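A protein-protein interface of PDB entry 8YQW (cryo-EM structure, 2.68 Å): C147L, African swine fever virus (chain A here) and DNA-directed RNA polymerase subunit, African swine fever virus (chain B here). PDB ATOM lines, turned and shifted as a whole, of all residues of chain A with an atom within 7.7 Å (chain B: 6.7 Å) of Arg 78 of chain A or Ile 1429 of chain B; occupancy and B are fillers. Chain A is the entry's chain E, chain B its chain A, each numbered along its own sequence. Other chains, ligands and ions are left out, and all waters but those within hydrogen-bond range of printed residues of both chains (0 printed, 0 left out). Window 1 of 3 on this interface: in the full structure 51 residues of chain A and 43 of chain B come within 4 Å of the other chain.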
ATOM      1  N   LEU A  71      -0.178  -6.634  -6.353  1.00  0.00           N
ATOM      2  CA  LEU A  71       0.366  -5.541  -7.141  1.00  0.00           C
ATOM      3  C   LEU A  71      -0.758  -4.686  -7.705  1.00  0.00           C
ATOM      4  O   LEU A  71      -1.785  -5.200  -8.152  1.00  0.00           O
ATOM      5  CB  LEU A  71       1.225  -6.083  -8.282  1.00  0.00           C
ATOM      6  CG  LEU A  71       2.582  -6.674  -7.925  1.00  0.00           C
ATOM      7  CD1 LEU A  71       3.028  -7.637  -9.004  1.00  0.00           C
ATOM      8  CD2 LEU A  71       3.593  -5.563  -7.732  1.00  0.00           C
ATOM      9  N   THR A  72      -0.563  -3.375  -7.677  1.00  0.00           N
ATOM     10  CA  THR A  72      -1.483  -2.509  -8.388  1.00  0.00           C
ATOM     11  C   THR A  72      -1.202  -2.597  -9.882  1.00  0.00           C
ATOM     12  O   THR A  72      -0.163  -3.100 -10.314  1.00  0.00           O
ATOM     13  CB  THR A  72      -1.369  -1.060  -7.905  1.00  0.00           C
ATOM     14  OG1 THR A  72      -0.135  -0.493  -8.353  1.00  0.00           O
ATOM     15  CG2 THR A  72      -1.416  -0.999  -6.394  1.00  0.00           C
ATOM     16  N   THR A  73      -2.155  -2.122 -10.678  1.00  0.00           N
ATOM     17  CA  THR A  73      -1.949  -2.106 -12.120  1.00  0.00           C
ATOM     18  C   THR A  73      -0.781  -1.200 -12.483  1.00  0.00           C
ATOM     19  O   THR A  73       0.000  -1.512 -13.390  1.00  0.00           O
ATOM     20  CB  THR A  73      -3.228  -1.664 -12.827  1.00  0.00           C
ATOM     21  OG1 THR A  73      -4.306  -2.516 -12.426  1.00  0.00           O
ATOM     22  CG2 THR A  73      -3.068  -1.772 -14.324  1.00  0.00           C
ATOM     23  N   PHE A  74      -0.635  -0.084 -11.766  1.00  0.00           N
ATOM     24  CA  PHE A  74       0.509   0.799 -11.967  1.00  0.00           C
ATOM     25  C   PHE A  74       1.819   0.078 -11.671  1.00  0.00           C
ATOM     26  O   PHE A  74       2.782   0.177 -12.436  1.00  0.00           O
ATOM     27  CB  PHE A  74       0.376   2.033 -11.076  1.00  0.00           C
ATOM     28  CG  PHE A  74      -0.781   2.916 -11.422  1.00  0.00           C
ATOM     29  CD1 PHE A  74      -1.146   3.125 -12.735  1.00  0.00           C
ATOM     30  CD2 PHE A  74      -1.498   3.551 -10.425  1.00  0.00           C
ATOM     31  CE1 PHE A  74      -2.207   3.941 -13.045  1.00  0.00           C
ATOM     32  CE2 PHE A  74      -2.558   4.367 -10.732  1.00  0.00           C
ATOM     33  CZ  PHE A  74      -2.912   4.562 -12.044  1.00  0.00           C
ATOM     34  N   GLU A  75       1.866  -0.661 -10.560  1.00  0.00           N
ATOM     35  CA  GLU A  75       3.097  -1.341 -10.171  1.00  0.00           C
ATOM     36  C   GLU A  75       3.451  -2.459 -11.140  1.00  0.00           C
ATOM     37  O   GLU A  75       4.619  -2.618 -11.508  1.00  0.00           O
ATOM     38  CB  GLU A  75       2.972  -1.883  -8.749  1.00  0.00           C
ATOM     39  CG  GLU A  75       3.174  -0.835  -7.677  1.00  0.00           C
ATOM     40  CD  GLU A  75       2.703  -1.287  -6.311  1.00  0.00           C
ATOM     41  OE1 GLU A  75       2.125  -2.387  -6.211  1.00  0.00           O
ATOM     42  OE2 GLU A  75       2.905  -0.536  -5.335  1.00  0.00           O
ATOM     43  N   ALA A  76       2.462  -3.252 -11.559  1.00  0.00           N
ATOM     44  CA  ALA A  76       2.729  -4.314 -12.523  1.00  0.00           C
ATOM     45  C   ALA A  76       3.171  -3.743 -13.864  1.00  0.00           C
ATOM     46  O   ALA A  76       4.097  -4.266 -14.495  1.00  0.00           O
ATOM     47  CB  ALA A  76       1.491  -5.190 -12.692  1.00  0.00           C
ATOM     48  N   THR A  77       2.523  -2.666 -14.312  1.00  0.00           N
ATOM     49  CA  THR A  77       2.929  -2.018 -15.554  1.00  0.00           C
ATOM     50  C   THR A  77       4.356  -1.501 -15.464  1.00  0.00           C
ATOM     51  O   THR A  77       5.150  -1.682 -16.394  1.00  0.00           O
ATOM     52  CB  THR A  77       1.965  -0.880 -15.884  1.00  0.00           C
ATOM     53  OG1 THR A  77       0.628  -1.387 -15.943  1.00  0.00           O
ATOM     54  CG2 THR A  77       2.313  -0.247 -17.213  1.00  0.00           C
ATOM     55  N   ARG A  78       4.704  -0.863 -14.345  1.00  0.00           N
ATOM     56  CA  ARG A  78       6.058  -0.353 -14.163  1.00  0.00           C
ATOM     57  C   ARG A  78       7.081  -1.480 -14.127  1.00  0.00           C
ATOM     58  O   ARG A  78       8.161  -1.366 -14.715  1.00  0.00           O
ATOM     59  CB  ARG A  78       6.124   0.477 -12.883  1.00  0.00           C
ATOM     60  CG  ARG A  78       7.507   0.931 -12.499  1.00  0.00           C
ATOM     61  CD  ARG A  78       7.996   2.068 -13.373  1.00  0.00           C
ATOM     62  NE  ARG A  78       9.201   2.666 -12.814  1.00  0.00           N
ATOM     63  CZ  ARG A  78      10.116   3.312 -13.520  1.00  0.00           C
ATOM     64  NH1 ARG A  78       9.994   3.475 -14.825  1.00  0.00           N
ATOM     65  NH2 ARG A  78      11.185   3.801 -12.899  1.00  0.00           N
ATOM     66  N   LEU A  79       6.758  -2.578 -13.441  1.00  0.00           N
ATOM     67  CA  LEU A  79       7.665  -3.719 -13.386  1.00  0.00           C
ATOM     68  C   LEU A  79       7.910  -4.289 -14.774  1.00  0.00           C
ATOM     69  O   LEU A  79       9.057  -4.547 -15.161  1.00  0.00           O
ATOM     70  CB  LEU A  79       7.094  -4.796 -12.465  1.00  0.00           C
ATOM     71  CG  LEU A  79       7.245  -4.602 -10.960  1.00  0.00           C
ATOM     72  CD1 LEU A  79       6.317  -5.544 -10.226  1.00  0.00           C
ATOM     73  CD2 LEU A  79       8.676  -4.831 -10.536  1.00  0.00           C
ATOM     74  N   VAL A  80       6.838  -4.484 -15.545  1.00  0.00           N
ATOM     75  CA  VAL A  80       6.984  -5.044 -16.884  1.00  0.00           C
ATOM     76  C   VAL A  80       7.778  -4.101 -17.775  1.00  0.00           C
ATOM     77  O   VAL A  80       8.641  -4.537 -18.543  1.00  0.00           O
ATOM     78  CB  VAL A  80       5.604  -5.371 -17.485  1.00  0.00           C
ATOM     79  CG1 VAL A  80       5.736  -5.750 -18.944  1.00  0.00           C
ATOM     80  CG2 VAL A  80       4.957  -6.495 -16.718  1.00  0.00           C
ATOM     81  N   ALA A  81       7.513  -2.795 -17.685  1.00  0.00           N
ATOM     82  CA  ALA A  81       8.229  -1.839 -18.524  1.00  0.00           C
ATOM     83  C   ALA A  81       9.715  -1.804 -18.192  1.00  0.00           C
ATOM     84  O   ALA A  81      10.562  -1.808 -19.095  1.00  0.00           O
ATOM     85  CB  ALA A  81       7.615  -0.448 -18.370  1.00  0.00           C
ATOM     86  N   VAL A  82      10.052  -1.773 -16.901  1.00  0.00           N
ATOM     87  CA  VAL A  82      11.454  -1.746 -16.497  1.00  0.00           C
ATOM     88  C   VAL A  82      12.158  -3.022 -16.933  1.00  0.00           C
ATOM     89  O   VAL A  82      13.276  -2.984 -17.462  1.00  0.00           O
ATOM     90  CB  VAL A  82      11.567  -1.524 -14.978  1.00  0.00           C
ATOM     91  CG1 VAL A  82      12.975  -1.808 -14.499  1.00  0.00           C
ATOM     92  CG2 VAL A  82      11.163  -0.108 -14.624  1.00  0.00           C
ATOM     93  N   ARG A  83      11.513  -4.174 -16.728  1.00  0.00           N
ATOM     94  CA  ARG A  83      12.122  -5.438 -17.122  1.00  0.00           C
ATOM     95  C   ARG A  83      12.309  -5.518 -18.631  1.00  0.00           C
ATOM     96  O   ARG A  83      13.329  -6.022 -19.108  1.00  0.00           O
ATOM     97  CB  ARG A  83      11.274  -6.603 -16.624  1.00  0.00           C
ATOM     98  CG  ARG A  83      11.913  -7.955 -16.832  1.00  0.00           C
ATOM     99  CD  ARG A  83      13.308  -7.985 -16.249  1.00  0.00           C
ATOM    100  NE  ARG A  83      14.080  -9.117 -16.741  1.00  0.00           N
ATOM    101  CZ  ARG A  83      15.403  -9.162 -16.769  1.00  0.00           C
ATOM    102  NH1 ARG A  83      16.137  -8.153 -16.330  1.00  0.00           N
ATOM    103  NH2 ARG A  83      16.005 -10.246 -17.246  1.00  0.00           N
ATOM    104  N   ALA A  84      11.335  -5.029 -19.399  1.00  0.00           N
ATOM    105  CA  ALA A  84      11.453  -5.053 -20.851  1.00  0.00           C
ATOM    106  C   ALA A  84      12.586  -4.160 -21.333  1.00  0.00           C
ATOM    107  O   ALA A  84      13.341  -4.540 -22.235  1.00  0.00           O
ATOM    108  CB  ALA A  84      10.130  -4.636 -21.488  1.00  0.00           C
ATOM    109  N   GLN A  86      15.272  -3.335 -19.590  1.00  0.00           N
ATOM    110  CA  GLN A  86      16.524  -3.969 -19.195  1.00  0.00           C
ATOM    111  C   GLN A  86      16.845  -5.180 -20.062  1.00  0.00           C
ATOM    112  O   GLN A  86      18.020  -5.476 -20.294  1.00  0.00           O
ATOM    113  CB  GLN A  86      16.463  -4.355 -17.723  1.00  0.00           C
ATOM    114  CG  GLN A  86      16.522  -3.161 -16.799  1.00  0.00           C
ATOM    115  CD  GLN A  86      16.322  -3.542 -15.361  1.00  0.00           C
ATOM    116  OE1 GLN A  86      16.006  -4.688 -15.049  1.00  0.00           O
ATOM    117  NE2 GLN A  86      16.502  -2.583 -14.468  1.00  0.00           N
ATOM    118  N   ILE A 115      10.689 -12.588 -12.164  1.00  0.00           N
ATOM    119  CA  ILE A 115      11.153 -11.242 -12.485  1.00  0.00           C
ATOM    120  C   ILE A 115      12.150 -10.782 -11.425  1.00  0.00           C
ATOM    121  O   ILE A 115      11.854 -10.844 -10.223  1.00  0.00           O
ATOM    122  CB  ILE A 115       9.961 -10.281 -12.631  1.00  0.00           C
ATOM    123  CG1 ILE A 115      10.428  -8.871 -12.983  1.00  0.00           C
ATOM    124  CG2 ILE A 115       9.084 -10.294 -11.386  1.00  0.00           C
ATOM    125  CD1 ILE A 115       9.379  -8.063 -13.700  1.00  0.00           C
ATOM    126  N   PRO A 116      13.349 -10.346 -11.815  1.00  0.00           N
ATOM    127  CA  PRO A 116      14.388  -9.983 -10.838  1.00  0.00           C
ATOM    128  C   PRO A 116      14.292  -8.527 -10.383  1.00  0.00           C
ATOM    129  O   PRO A 116      15.236  -7.745 -10.510  1.00  0.00           O
ATOM    130  CB  PRO A 116      15.673 -10.259 -11.622  1.00  0.00           C
ATOM    131  CG  PRO A 116      15.308  -9.910 -13.016  1.00  0.00           C
ATOM    132  CD  PRO A 116      13.849 -10.257 -13.196  1.00  0.00           C
ATOM    133  N   LEU A 117      13.138  -8.160  -9.834  1.00  0.00           N
ATOM    134  CA  LEU A 117      12.892  -6.802  -9.377  1.00  0.00           C
ATOM    135  C   LEU A 117      12.153  -6.851  -8.049  1.00  0.00           C
ATOM    136  O   LEU A 117      11.556  -7.867  -7.689  1.00  0.00           O
ATOM    137  CB  LEU A 117      12.085  -5.997 -10.403  1.00  0.00           C
ATOM    138  CG  LEU A 117      12.699  -5.797 -11.789  1.00  0.00           C
ATOM    139  CD1 LEU A 117      11.696  -5.163 -12.730  1.00  0.00           C
ATOM    140  CD2 LEU A 117      13.946  -4.951 -11.697  1.00  0.00           C
ATOM    141  N   LEU A 118      12.211  -5.744  -7.316  1.00  0.00           N
ATOM    142  CA  LEU A 118      11.501  -5.606  -6.053  1.00  0.00           C
ATOM    143  C   LEU A 118      10.741  -4.290  -6.039  1.00  0.00           C
ATOM    144  O   LEU A 118      11.166  -3.301  -6.639  1.00  0.00           O
ATOM    145  CB  LEU A 118      12.455  -5.663  -4.855  1.00  0.00           C
ATOM    146  CG  LEU A 118      13.149  -6.987  -4.539  1.00  0.00           C
ATOM    147  CD1 LEU A 118      14.006  -6.843  -3.299  1.00  0.00           C
ATOM    148  CD2 LEU A 118      12.136  -8.096  -4.356  1.00  0.00           C
ATOM    149  N   VAL A 119       9.608  -4.284  -5.347  1.00  0.00           N
ATOM    150  CA  VAL A 119       8.790  -3.088  -5.187  1.00  0.00           C
ATOM    151  C   VAL A 119       9.081  -2.497  -3.818  1.00  0.00           C
ATOM    152  O   VAL A 119       8.903  -3.169  -2.794  1.00  0.00           O
ATOM    153  CB  VAL A 119       7.293  -3.400  -5.344  1.00  0.00           C
ATOM    154  CG1 VAL A 119       6.479  -2.125  -5.262  1.00  0.00           C
ATOM    155  CG2 VAL A 119       7.036  -4.118  -6.653  1.00  0.00           C
ATOM    156  N   MET A 120       9.528  -1.249  -3.792  1.00  0.00           N
ATOM    157  CA  MET A 120       9.772  -0.528  -2.549  1.00  0.00           C
ATOM    158  C   MET A 120       8.706   0.549  -2.414  1.00  0.00           C
ATOM    159  O   MET A 120       8.661   1.491  -3.211  1.00  0.00           O
ATOM    160  CB  MET A 120      11.173   0.073  -2.526  1.00  0.00           C
ATOM    161  CG  MET A 120      11.448   0.952  -1.322  1.00  0.00           C
ATOM    162  SD  MET A 120      13.173   1.455  -1.223  1.00  0.00           S
ATOM    163  CE  MET A 120      13.067   3.124  -1.853  1.00  0.00           C
ATOM    164  N   ARG A 121       7.849   0.405  -1.412  1.00  0.00           N
ATOM    165  CA  ARG A 121       6.763   1.345  -1.157  1.00  0.00           C
ATOM    166  C   ARG A 121       7.213   2.278  -0.040  1.00  0.00           C
ATOM    167  O   ARG A 121       7.269   1.886   1.126  1.00  0.00           O
ATOM    168  CB  ARG A 121       5.482   0.600  -0.799  1.00  0.00           C
ATOM    169  CG  ARG A 121       4.924  -0.225  -1.941  1.00  0.00           C
ATOM    170  CD  ARG A 121       3.757  -1.082  -1.504  1.00  0.00           C
ATOM    171  NE  ARG A 121       3.087  -1.691  -2.645  1.00  0.00           N
ATOM    172  CZ  ARG A 121       2.266  -2.728  -2.568  1.00  0.00           C
ATOM    173  NH1 ARG A 121       1.992  -3.308  -1.415  1.00  0.00           N
ATOM    174  NH2 ARG A 121       1.710  -3.197  -3.680  1.00  0.00           N
ATOM    175  N   PRO A 138       7.645  -9.119  -5.912  1.00  0.00           N
ATOM    176  CA  PRO A 138       6.564  -9.374  -6.874  1.00  0.00           C
ATOM    177  C   PRO A 138       6.483 -10.812  -7.352  1.00  0.00           C
ATOM    178  O   PRO A 138       5.518 -11.160  -8.039  1.00  0.00           O
ATOM    179  CB  PRO A 138       6.901  -8.427  -8.032  1.00  0.00           C
ATOM    180  CG  PRO A 138       8.353  -8.214  -7.929  1.00  0.00           C
ATOM    181  CD  PRO A 138       8.684  -8.244  -6.471  1.00  0.00           C
ATOM    182  N   LEU A 145      -2.733  -8.381 -13.910  1.00  0.00           N
ATOM    183  CA  LEU A 145      -2.807  -8.407 -15.363  1.00  0.00           C
ATOM    184  C   LEU A 145      -3.235  -9.786 -15.867  1.00  0.00           C
ATOM    185  O   LEU A 145      -3.216 -10.784 -15.141  1.00  0.00           O
ATOM    186  CB  LEU A 145      -1.463  -8.012 -15.971  1.00  0.00           C
ATOM    187  CG  LEU A 145      -0.831  -6.733 -15.420  1.00  0.00           C
ATOM    188  CD1 LEU A 145       0.597  -6.607 -15.910  1.00  0.00           C
ATOM    189  CD2 LEU A 145      -1.649  -5.510 -15.801  1.00  0.00           C
ATOM    190  N   MET B 472       9.291   1.331 -22.897  1.00  0.00           N
ATOM    191  CA  MET B 472       8.587   1.666 -21.661  1.00  0.00           C
ATOM    192  C   MET B 472       7.214   2.264 -21.939  1.00  0.00           C
ATOM    193  O   MET B 472       6.230   1.903 -21.286  1.00  0.00           O
ATOM    194  CB  MET B 472       9.426   2.631 -20.830  1.00  0.00           C
ATOM    195  CG  MET B 472      10.630   2.006 -20.168  1.00  0.00           C
ATOM    196  SD  MET B 472      11.023   2.812 -18.613  1.00  0.00           S
ATOM    197  CE  MET B 472      12.128   1.618 -17.887  1.00  0.00           C
ATOM    198  N   VAL B 475       4.935  -0.520 -23.487  1.00  0.00           N
ATOM    199  CA  VAL B 475       4.355  -1.408 -22.480  1.00  0.00           C
ATOM    200  C   VAL B 475       3.181  -0.724 -21.795  1.00  0.00           C
ATOM    201  O   VAL B 475       2.115  -1.319 -21.595  1.00  0.00           O
ATOM    202  CB  VAL B 475       5.421  -1.827 -21.452  1.00  0.00           C
ATOM    203  CG1 VAL B 475       4.760  -2.430 -20.227  1.00  0.00           C
ATOM    204  CG2 VAL B 475       6.398  -2.799 -22.059  1.00  0.00           C
ATOM    205  N   GLU B 476       3.363   0.541 -21.429  1.00  0.00           N
ATOM    206  CA  GLU B 476       2.348   1.286 -20.700  1.00  0.00           C
ATOM    207  C   GLU B 476       1.091   1.511 -21.525  1.00  0.00           C
ATOM    208  O   GLU B 476       0.001   1.605 -20.954  1.00  0.00           O
ATOM    209  CB  GLU B 476       2.932   2.623 -20.261  1.00  0.00           C
ATOM    210  CG  GLU B 476       2.334   3.189 -19.011  1.00  0.00           C
ATOM    211  CD  GLU B 476       2.902   4.544 -18.701  1.00  0.00           C
ATOM    212  OE1 GLU B 476       3.331   5.226 -19.652  1.00  0.00           O
ATOM    213  OE2 GLU B 476       2.947   4.917 -17.511  1.00  0.00           O
ATOM    214  N   LEU B 479      -0.928  -1.993 -21.230  1.00  0.00           N
ATOM    215  CA  LEU B 479      -1.415  -2.456 -19.937  1.00  0.00           C
ATOM    216  C   LEU B 479      -2.325  -1.448 -19.250  1.00  0.00           C
ATOM    217  O   LEU B 479      -3.257  -1.850 -18.546  1.00  0.00           O
ATOM    218  CB  LEU B 479      -0.232  -2.799 -19.033  1.00  0.00           C
ATOM    219  CG  LEU B 479       0.696  -3.896 -19.559  1.00  0.00           C
ATOM    220  CD1 LEU B 479       1.671  -4.337 -18.488  1.00  0.00           C
ATOM    221  CD2 LEU B 479      -0.102  -5.077 -20.073  1.00  0.00           C
ATOM    222  N   LEU B 480      -2.087  -0.152 -19.432  1.00  0.00           N
ATOM    223  CA  LEU B 480      -2.883   0.876 -18.774  1.00  0.00           C
ATOM    224  C   LEU B 480      -3.868   1.569 -19.698  1.00  0.00           C
ATOM    225  O   LEU B 480      -5.043   1.709 -19.354  1.00  0.00           O
ATOM    226  CB  LEU B 480      -1.981   1.941 -18.137  1.00  0.00           C
ATOM    227  CG  LEU B 480      -1.225   1.648 -16.852  1.00  0.00           C
ATOM    228  CD1 LEU B 480      -0.362   2.837 -16.528  1.00  0.00           C
ATOM    229  CD2 LEU B 480      -2.196   1.380 -15.730  1.00  0.00           C
ATOM    230  N   GLY B1423       1.030   7.380 -10.325  1.00  0.00           N
ATOM    231  CA  GLY B1423       0.741   6.256 -11.191  1.00  0.00           C
ATOM    232  C   GLY B1423       1.858   5.240 -11.261  1.00  0.00           C
ATOM    233  O   GLY B1423       2.209   4.626 -10.252  1.00  0.00           O
ATOM    234  N   THR B1424       2.421   5.047 -12.455  1.00  0.00           N
ATOM    235  CA  THR B1424       3.525   4.108 -12.608  1.00  0.00           C
ATOM    236  C   THR B1424       4.788   4.581 -11.908  1.00  0.00           C
ATOM    237  O   THR B1424       5.654   3.758 -11.601  1.00  0.00           O
ATOM    238  CB  THR B1424       3.818   3.864 -14.087  1.00  0.00           C
ATOM    239  OG1 THR B1424       4.002   5.115 -14.755  1.00  0.00           O
ATOM    240  CG2 THR B1424       2.679   3.116 -14.734  1.00  0.00           C
ATOM    241  N   MET B1425       4.911   5.878 -11.643  1.00  0.00           N
ATOM    242  CA  MET B1425       6.067   6.429 -10.954  1.00  0.00           C
ATOM    243  C   MET B1425       5.885   6.498  -9.445  1.00  0.00           C
ATOM    244  O   MET B1425       6.792   6.969  -8.753  1.00  0.00           O
ATOM    245  CB  MET B1425       6.377   7.833 -11.477  1.00  0.00           C
ATOM    246  CG  MET B1425       6.709   7.914 -12.951  1.00  0.00           C
ATOM    247  SD  MET B1425       8.191   7.023 -13.433  1.00  0.00           S
ATOM    248  CE  MET B1425       7.477   5.668 -14.346  1.00  0.00           C
ATOM    249  N   SER B1427       5.465   4.069  -6.986  1.00  0.00           N
ATOM    250  CA  SER B1427       6.339   3.132  -6.296  1.00  0.00           C
ATOM    251  C   SER B1427       7.614   2.962  -7.105  1.00  0.00           C
ATOM    252  O   SER B1427       7.560   2.808  -8.329  1.00  0.00           O
ATOM    253  CB  SER B1427       5.654   1.781  -6.097  1.00  0.00           C
ATOM    254  OG  SER B1427       4.460   1.916  -5.350  1.00  0.00           O
ATOM    255  N   ASP B1428       8.754   2.994  -6.428  1.00  0.00           N
ATOM    256  CA  ASP B1428      10.035   2.866  -7.099  1.00  0.00           C
ATOM    257  C   ASP B1428      10.495   1.414  -7.106  1.00  0.00           C
ATOM    258  O   ASP B1428      10.175   0.634  -6.208  1.00  0.00           O
ATOM    259  CB  ASP B1428      11.088   3.777  -6.457  1.00  0.00           C
ATOM    260  CG  ASP B1428      11.192   3.601  -4.959  1.00  0.00           C
ATOM    261  OD1 ASP B1428      11.118   2.460  -4.476  1.00  0.00           O
ATOM    262  OD2 ASP B1428      11.351   4.619  -4.256  1.00  0.00           O
ATOM    263  N   ILE B1429      11.227   1.053  -8.152  1.00  0.00           N
ATOM    264  CA  ILE B1429      11.684  -0.313  -8.368  1.00  0.00           C
ATOM    265  C   ILE B1429      13.154  -0.395  -7.998  1.00  0.00           C
ATOM    266  O   ILE B1429      13.933   0.518  -8.294  1.00  0.00           O
ATOM    267  CB  ILE B1429      11.454  -0.753  -9.826  1.00  0.00           C
ATOM    268  CG1 ILE B1429      10.049  -0.371 -10.290  1.00  0.00           C
ATOM    269  CG2 ILE B1429      11.657  -2.243  -9.970  1.00  0.00           C
ATOM    270  CD1 ILE B1429       8.943  -0.978  -9.467  1.00  0.00           C
ATOM    271  N   ILE B1430      13.534  -1.478  -7.329  1.00  0.00           N
ATOM    272  CA  ILE B1430      14.928  -1.743  -7.007  1.00  0.00           C
ATOM    273  C   ILE B1430      15.279  -3.132  -7.513  1.00  0.00           C
ATOM    274  O   ILE B1430      14.442  -4.038  -7.536  1.00  0.00           O
ATOM    275  CB  ILE B1430      15.224  -1.615  -5.495  1.00  0.00           C
ATOM    276  CG1 ILE B1430      14.479  -2.683  -4.700  1.00  0.00           C
ATOM    277  CG2 ILE B1430      14.848  -0.242  -4.996  1.00  0.00           C
ATOM    278  CD1 ILE B1430      14.884  -2.752  -3.259  1.00  0.00           C
ATOM    279  N   MET B1431      16.527  -3.290  -7.940  1.00  0.00           N
ATOM    280  CA  MET B1431      16.994  -4.564  -8.460  1.00  0.00           C
ATOM    281  C   MET B1431      17.071  -5.589  -7.337  1.00  0.00           C
ATOM    282  O   MET B1431      17.527  -5.286  -6.233  1.00  0.00           O
ATOM    283  CB  MET B1431      18.362  -4.401  -9.115  1.00  0.00           C
ATOM    284  CG  MET B1431      18.376  -3.470 -10.312  1.00  0.00           C
ATOM    285  SD  MET B1431      17.337  -4.004 -11.677  1.00  0.00           S
ATOM    286  CE  MET B1431      17.937  -5.663 -11.937  1.00  0.00           C
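Of the printed residues of chain B, Phe 74 of chain A touches Leu 480, Gly 1423 and Thr 1424.
Of the printed residues of chain B, Arg 78 of chain A touches Met 472, Thr 1424, Met 1425 and Ile 1429.
Of the printed residues of chain B, Leu 79 of chain A touches Ile 1429 (3.99 Å).
Printed residues of chain B within 4 Å of Leu 117 of chain A: Ile 1429 (3.8 Å), Ile 1430 (3.7 Å) and Met 1431 (3.5 Å).
Printed residues of chain B that touch a printed residue of chain A: Met 472, Val 475, Glu 476, Leu 479, Leu 480, Gly 1423, Thr 1424, Met 1425, Ser 1427, Asp 1428, Ile 1429, Ile 1430 and Met 1431.
Of the 24 printed residues of chain A, 15 touch a printed residue of chain B.
Printed residues of chain A that touch a printed residue of chain B: Thr 73, Phe 74, Glu 75, Thr 77, Arg 78, Leu 79, Val 80, Ala 81, Val 82, Gln 86, Pro 116, Leu 117, Leu 118, Met 120 and Leu 145.
Hydrophobic or aromatic side chains of chain A that line the printed part of chain B: Phe 74, Leu 79, Val 80, Ala 81, Val 82, Leu 117, Leu 118, Met 120 and Leu 145.
Among the printed residues, no Asp or Glu carboxylate lies within 4 Å of a Lys or Arg side-chain nitrogen of the other chain.
NE2 of Gln 86 of chain A is in hydrogen-bond range of SD of Met 1431 of chain B, at 3.2 Å.
The side-chain hydroxyl (OG) of Ser 1427 of chain B is in hydrogen-bond range of the side-chain carboxylate (OE2) of Glu 75 of chain A (2.9 Å).
The backbone carbonyl oxygen of Asp 1428 of chain B sits at hydrogen-bond distance from the backbone NH of Met 120 of chain A (3.1 Å).
The backbone carbonyl oxygen (O) of Ile 1430 of chain B sits at hydrogen-bond distance from the backbone NH (N) of Leu 118 of chain A.
CG2 of Thr 73 of chain A touches CD2 of Leu 480 of chain B (3.6 Å).
Thr 77 of chain A touches Glu 476 of chain B.
Thr 77 of chain A touches Leu 479 of chain B (OG1 to CB, 3.5 Å).
NH1 of Arg 78 of chain A touches SD of Met 472 of chain B, at 3.98 Å.
Arg 78 of chain A touches Ile 1429 of chain B.
O of Ala 81 of chain A touches CE of Met 472 of chain B (3.96 Å).
N of Ala 81 of chain A touches CG1 of Val 475 of chain B (3.8 Å).
Leu 117 of chain A touches Ile 1429 of chain B (CB to CG2, 3.8 Å).
Leu 117 of chain A touches Ile 1430 of chain B.
Leu 479 of chain B touches Leu 145 of chain A (CD1 to CD1, 3.6 Å).
The guanidinium group (NH2) of Arg 121 of chain A lies within salt-bridge range of the side-chain carboxylate (OE1) of Glu 75 of chain A, at 2.7 Å.
The side-chain hydroxyl (OG1) of Thr 72 of chain A sits at hydrogen-bond distance from the backbone NH (N) of Glu 75 of chain A, at 3.0 Å.
OG1 of Thr 77 of chain A is in hydrogen-bond range of O of Thr 73 of chain A (2.6 Å).
The side-chain hydroxyl (OG1) of Thr 72 of chain A lies close to the backbone NH (N) of Phe 74 of chain A (3.5 Å).
The side-chain carboxylate (OE2) of Glu 476 of chain B sits at hydrogen-bond distance from the side-chain hydroxyl (OG1) of Thr 1424 of chain B (3.0 Å).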
